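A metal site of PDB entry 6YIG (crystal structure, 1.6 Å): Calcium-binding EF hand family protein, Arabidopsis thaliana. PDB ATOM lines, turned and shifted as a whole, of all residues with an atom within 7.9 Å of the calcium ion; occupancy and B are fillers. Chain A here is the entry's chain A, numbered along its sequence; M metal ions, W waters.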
ATOM      1  N   PHE A  17     -20.558  24.484 -26.362  1.00  0.00           N
ATOM      2  CA  PHE A  17     -19.950  23.223 -26.781  1.00  0.00           C
ATOM      3  C   PHE A  17     -18.831  22.815 -25.831  1.00  0.00           C
ATOM      4  O   PHE A  17     -18.748  21.665 -25.399  1.00  0.00           O
ATOM      5  CB  PHE A  17     -19.457  23.393 -28.236  1.00  0.00           C
ATOM      6  CG  PHE A  17     -18.901  22.158 -28.893  1.00  0.00           C
ATOM      7  CD1 PHE A  17     -19.647  21.010 -29.029  1.00  0.00           C
ATOM      8  CD2 PHE A  17     -17.653  22.204 -29.492  1.00  0.00           C
ATOM      9  CE1 PHE A  17     -19.155  19.902 -29.662  1.00  0.00           C
ATOM     10  CE2 PHE A  17     -17.140  21.093 -30.134  1.00  0.00           C
ATOM     11  CZ  PHE A  17     -17.900  19.918 -30.205  1.00  0.00           C
ATOM     12  N   ALA A  20     -20.330  21.705 -22.519  1.00  0.00           N
ATOM     13  CA  ALA A  20     -21.029  20.428 -22.594  1.00  0.00           C
ATOM     14  C   ALA A  20     -20.079  19.255 -22.744  1.00  0.00           C
ATOM     15  O   ALA A  20     -20.414  18.134 -22.322  1.00  0.00           O
ATOM     16  CB  ALA A  20     -22.012  20.449 -23.770  1.00  0.00           C
ATOM     17  N   ASP A  21     -18.916  19.455 -23.349  1.00  0.00           N
ATOM     18  CA  ASP A  21     -17.994  18.373 -23.686  1.00  0.00           C
ATOM     19  C   ASP A  21     -17.104  18.065 -22.486  1.00  0.00           C
ATOM     20  O   ASP A  21     -15.930  18.396 -22.433  1.00  0.00           O
ATOM     21  CB  ASP A  21     -17.166  18.738 -24.900  1.00  0.00           C
ATOM     22  CG  ASP A  21     -16.255  17.617 -25.321  1.00  0.00           C
ATOM     23  OD1 ASP A  21     -16.504  16.468 -24.875  1.00  0.00           O
ATOM     24  OD2 ASP A  21     -15.270  17.904 -26.064  1.00  0.00           O
ATOM     25  N   LEU A  22     -17.678  17.372 -21.510  1.00  0.00           N
ATOM     26  CA  LEU A  22     -17.009  17.245 -20.221  1.00  0.00           C
ATOM     27  C   LEU A  22     -15.679  16.511 -20.321  1.00  0.00           C
ATOM     28  O   LEU A  22     -14.788  16.755 -19.498  1.00  0.00           O
ATOM     29  CB  LEU A  22     -17.925  16.519 -19.235  1.00  0.00           C
ATOM     30  CG  LEU A  22     -19.284  17.166 -18.944  1.00  0.00           C
ATOM     31  CD1 LEU A  22     -20.043  16.250 -18.012  1.00  0.00           C
ATOM     32  CD2 LEU A  22     -19.110  18.541 -18.353  1.00  0.00           C
ATOM     33  N   ASP A  23     -15.529  15.594 -21.267  1.00  0.00           N
ATOM     34  CA  ASP A  23     -14.285  14.841 -21.380  1.00  0.00           C
ATOM     35  C   ASP A  23     -13.362  15.392 -22.455  1.00  0.00           C
ATOM     36  O   ASP A  23     -12.272  14.846 -22.623  1.00  0.00           O
ATOM     37  CB  ASP A  23     -14.533  13.341 -21.616  1.00  0.00           C
ATOM     38  CG  ASP A  23     -15.314  13.025 -22.889  1.00  0.00           C
ATOM     39  OD1 ASP A  23     -15.618  13.895 -23.696  1.00  0.00           O
ATOM     40  OD2 ASP A  23     -15.714  11.820 -23.025  1.00  0.00           O
ATOM     41  N   GLY A  24     -13.746  16.449 -23.141  1.00  0.00           N
ATOM     42  CA  GLY A  24     -12.855  17.037 -24.128  1.00  0.00           C
ATOM     43  C   GLY A  24     -12.563  16.200 -25.344  1.00  0.00           C
ATOM     44  O   GLY A  24     -11.576  16.477 -26.058  1.00  0.00           O
ATOM     45  N   ASP A  25     -13.382  15.197 -25.637  1.00  0.00           N
ATOM     46  CA  ASP A  25     -13.102  14.348 -26.797  1.00  0.00           C
ATOM     47  C   ASP A  25     -13.620  14.946 -28.090  1.00  0.00           C
ATOM     48  O   ASP A  25     -13.445  14.329 -29.151  1.00  0.00           O
ATOM     49  CB  ASP A  25     -13.642  12.926 -26.585  1.00  0.00           C
ATOM     50  CG  ASP A  25     -15.123  12.824 -26.723  1.00  0.00           C
ATOM     51  OD1 ASP A  25     -15.828  13.852 -26.653  1.00  0.00           O
ATOM     52  OD2 ASP A  25     -15.618  11.667 -26.853  1.00  0.00           O
ATOM     53  N   GLY A  26     -14.160  16.161 -28.043  1.00  0.00           N
ATOM     54  CA  GLY A  26     -14.598  16.866 -29.233  1.00  0.00           C
ATOM     55  C   GLY A  26     -15.932  16.432 -29.743  1.00  0.00           C
ATOM     56  O   GLY A  26     -16.320  16.816 -30.854  1.00  0.00           O
ATOM     57  N   ARG A  27     -16.661  15.627 -28.974  1.00  0.00           N
ATOM     58  CA  ARG A  27     -17.997  15.141 -29.308  1.00  0.00           C
ATOM     59  C   ARG A  27     -18.895  15.294 -28.096  1.00  0.00           C
ATOM     60  O   ARG A  27     -18.438  15.208 -26.965  1.00  0.00           O
ATOM     61  CB  ARG A  27     -17.980  13.662 -29.703  1.00  0.00           C
ATOM     62  CG  ARG A  27     -16.964  13.246 -30.761  1.00  0.00           C
ATOM     63  CD  ARG A  27     -17.019  11.717 -30.917  1.00  0.00           C
ATOM     64  NE  ARG A  27     -16.553  11.029 -29.723  1.00  0.00           N
ATOM     65  CZ  ARG A  27     -16.390   9.707 -29.642  1.00  0.00           C
ATOM     66  NH1 ARG A  27     -16.667   8.946 -30.685  1.00  0.00           N
ATOM     67  NH2 ARG A  27     -15.951   9.147 -28.517  1.00  0.00           N
ATOM     68  N   ILE A  28     -20.199  15.486 -28.336  1.00  0.00           N
ATOM     69  CA  ILE A  28     -21.173  15.508 -27.246  1.00  0.00           C
ATOM     70  C   ILE A  28     -21.870  14.155 -27.230  1.00  0.00           C
ATOM     71  O   ILE A  28     -22.626  13.807 -28.144  1.00  0.00           O
ATOM     72  CB  ILE A  28     -22.184  16.650 -27.366  1.00  0.00           C
ATOM     73  CG1 ILE A  28     -21.499  17.999 -27.566  1.00  0.00           C
ATOM     74  CG2 ILE A  28     -23.105  16.655 -26.125  1.00  0.00           C
ATOM     75  CD1 ILE A  28     -20.441  18.325 -26.537  1.00  0.00           C
ATOM     76  N   SER A  29     -21.619  13.391 -26.176  1.00  0.00           N
ATOM     77  CA  SER A  29     -22.256  12.106 -25.992  1.00  0.00           C
ATOM     78  C   SER A  29     -23.689  12.276 -25.498  1.00  0.00           C
ATOM     79  O   SER A  29     -24.104  13.361 -25.079  1.00  0.00           O
ATOM     80  CB  SER A  29     -21.492  11.289 -24.973  1.00  0.00           C
ATOM     81  OG  SER A  29     -21.669  11.860 -23.690  1.00  0.00           O
ATOM     82  N   GLY A  30     -24.451  11.182 -25.582  1.00  0.00           N
ATOM     83  CA  GLY A  30     -25.813  11.212 -25.039  1.00  0.00           C
ATOM     84  C   GLY A  30     -25.860  11.687 -23.600  1.00  0.00           C
ATOM     85  O   GLY A  30     -26.684  12.521 -23.229  1.00  0.00           O
ATOM     86  N   GLU A  32     -23.660  13.445 -21.931  1.00  0.00           N
ATOM     87  CA  GLU A  32     -23.274  14.849 -21.874  1.00  0.00           C
ATOM     88  C   GLU A  32     -24.431  15.742 -22.271  1.00  0.00           C
ATOM     89  O   GLU A  32     -24.628  16.805 -21.681  1.00  0.00           O
ATOM     90  CB  GLU A  32     -22.057  15.079 -22.770  1.00  0.00           C
ATOM     91  CG  GLU A  32     -20.748  14.563 -22.168  1.00  0.00           C
ATOM     92  CD  GLU A  32     -19.573  14.578 -23.110  1.00  0.00           C
ATOM     93  OE1 GLU A  32     -19.770  14.750 -24.338  1.00  0.00           O
ATOM     94  OE2 GLU A  32     -18.434  14.405 -22.621  1.00  0.00           O
ATOM     95  N   PHE A  61     -23.314  10.318 -30.824  1.00  0.00           N
ATOM     96  CA  PHE A  61     -22.510  11.470 -30.501  1.00  0.00           C
ATOM     97  C   PHE A  61     -22.882  12.602 -31.449  1.00  0.00           C
ATOM     98  O   PHE A  61     -23.214  12.371 -32.609  1.00  0.00           O
ATOM     99  CB  PHE A  61     -21.020  11.189 -30.668  1.00  0.00           C
ATOM    100  CG  PHE A  61     -20.495  10.124 -29.755  1.00  0.00           C
ATOM    101  CD1 PHE A  61     -20.562   8.799 -30.123  1.00  0.00           C
ATOM    102  CD2 PHE A  61     -19.971  10.461 -28.527  1.00  0.00           C
ATOM    103  CE1 PHE A  61     -20.098   7.830 -29.284  1.00  0.00           C
ATOM    104  CE2 PHE A  61     -19.506   9.500 -27.676  1.00  0.00           C
ATOM    105  CZ  PHE A  61     -19.567   8.180 -28.055  1.00  0.00           C
ATOM    106  N   LEU A  62     -22.795  13.817 -30.939  1.00  0.00           N
ATOM    107  CA  LEU A  62     -22.967  15.009 -31.745  1.00  0.00           C
ATOM    108  C   LEU A  62     -21.623  15.653 -32.007  1.00  0.00           C
ATOM    109  O   LEU A  62     -20.856  15.901 -31.077  1.00  0.00           O
ATOM    110  CB  LEU A  62     -23.855  16.031 -31.059  1.00  0.00           C
ATOM    111  CG  LEU A  62     -25.209  15.527 -30.548  1.00  0.00           C
ATOM    112  CD1 LEU A  62     -25.926  16.700 -29.874  1.00  0.00           C
ATOM    113  CD2 LEU A  62     -26.047  14.900 -31.640  1.00  0.00           C
HETATM  114 CA    CA M   1     -17.465  14.414 -25.040  1.00  0.00          CA
HETATM  115  O   HOH W   1     -18.028  12.161 -25.506  1.00  0.00           O
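The backbone NH of Gly 26 is in hydrogen-bond range of the side-chain carboxylate of Asp 21.
The side-chain hydroxyl (OG) of Ser 29 is in hydrogen-bond range of the backbone NH (N) of Glu 32 (3.1 Å).
OD1 of Asp 21 lies close to N of Gly 24.
The backbone NH (N) of Leu 22 sits close to the side-chain carboxylate (OE2) of Glu 32.
Within 4 Å of the calcium ion: Asp 21, Asp 23, Asp 25, Arg 27 and Glu 32.
Water W1 lies within hydrogen-bond range of OD2 of Asp 25 (2.8 Å) and OD2 of Asp 23 (3.4 Å).
The calcium ion is bound by OD1 of Asp 21, O of Arg 27, OD1 of Asp 23, OD1 of Asp 25, water W1, OE1 of Glu 32 and OE2 of Glu 32.
The calcium ion has seven donor atoms within binding distance.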
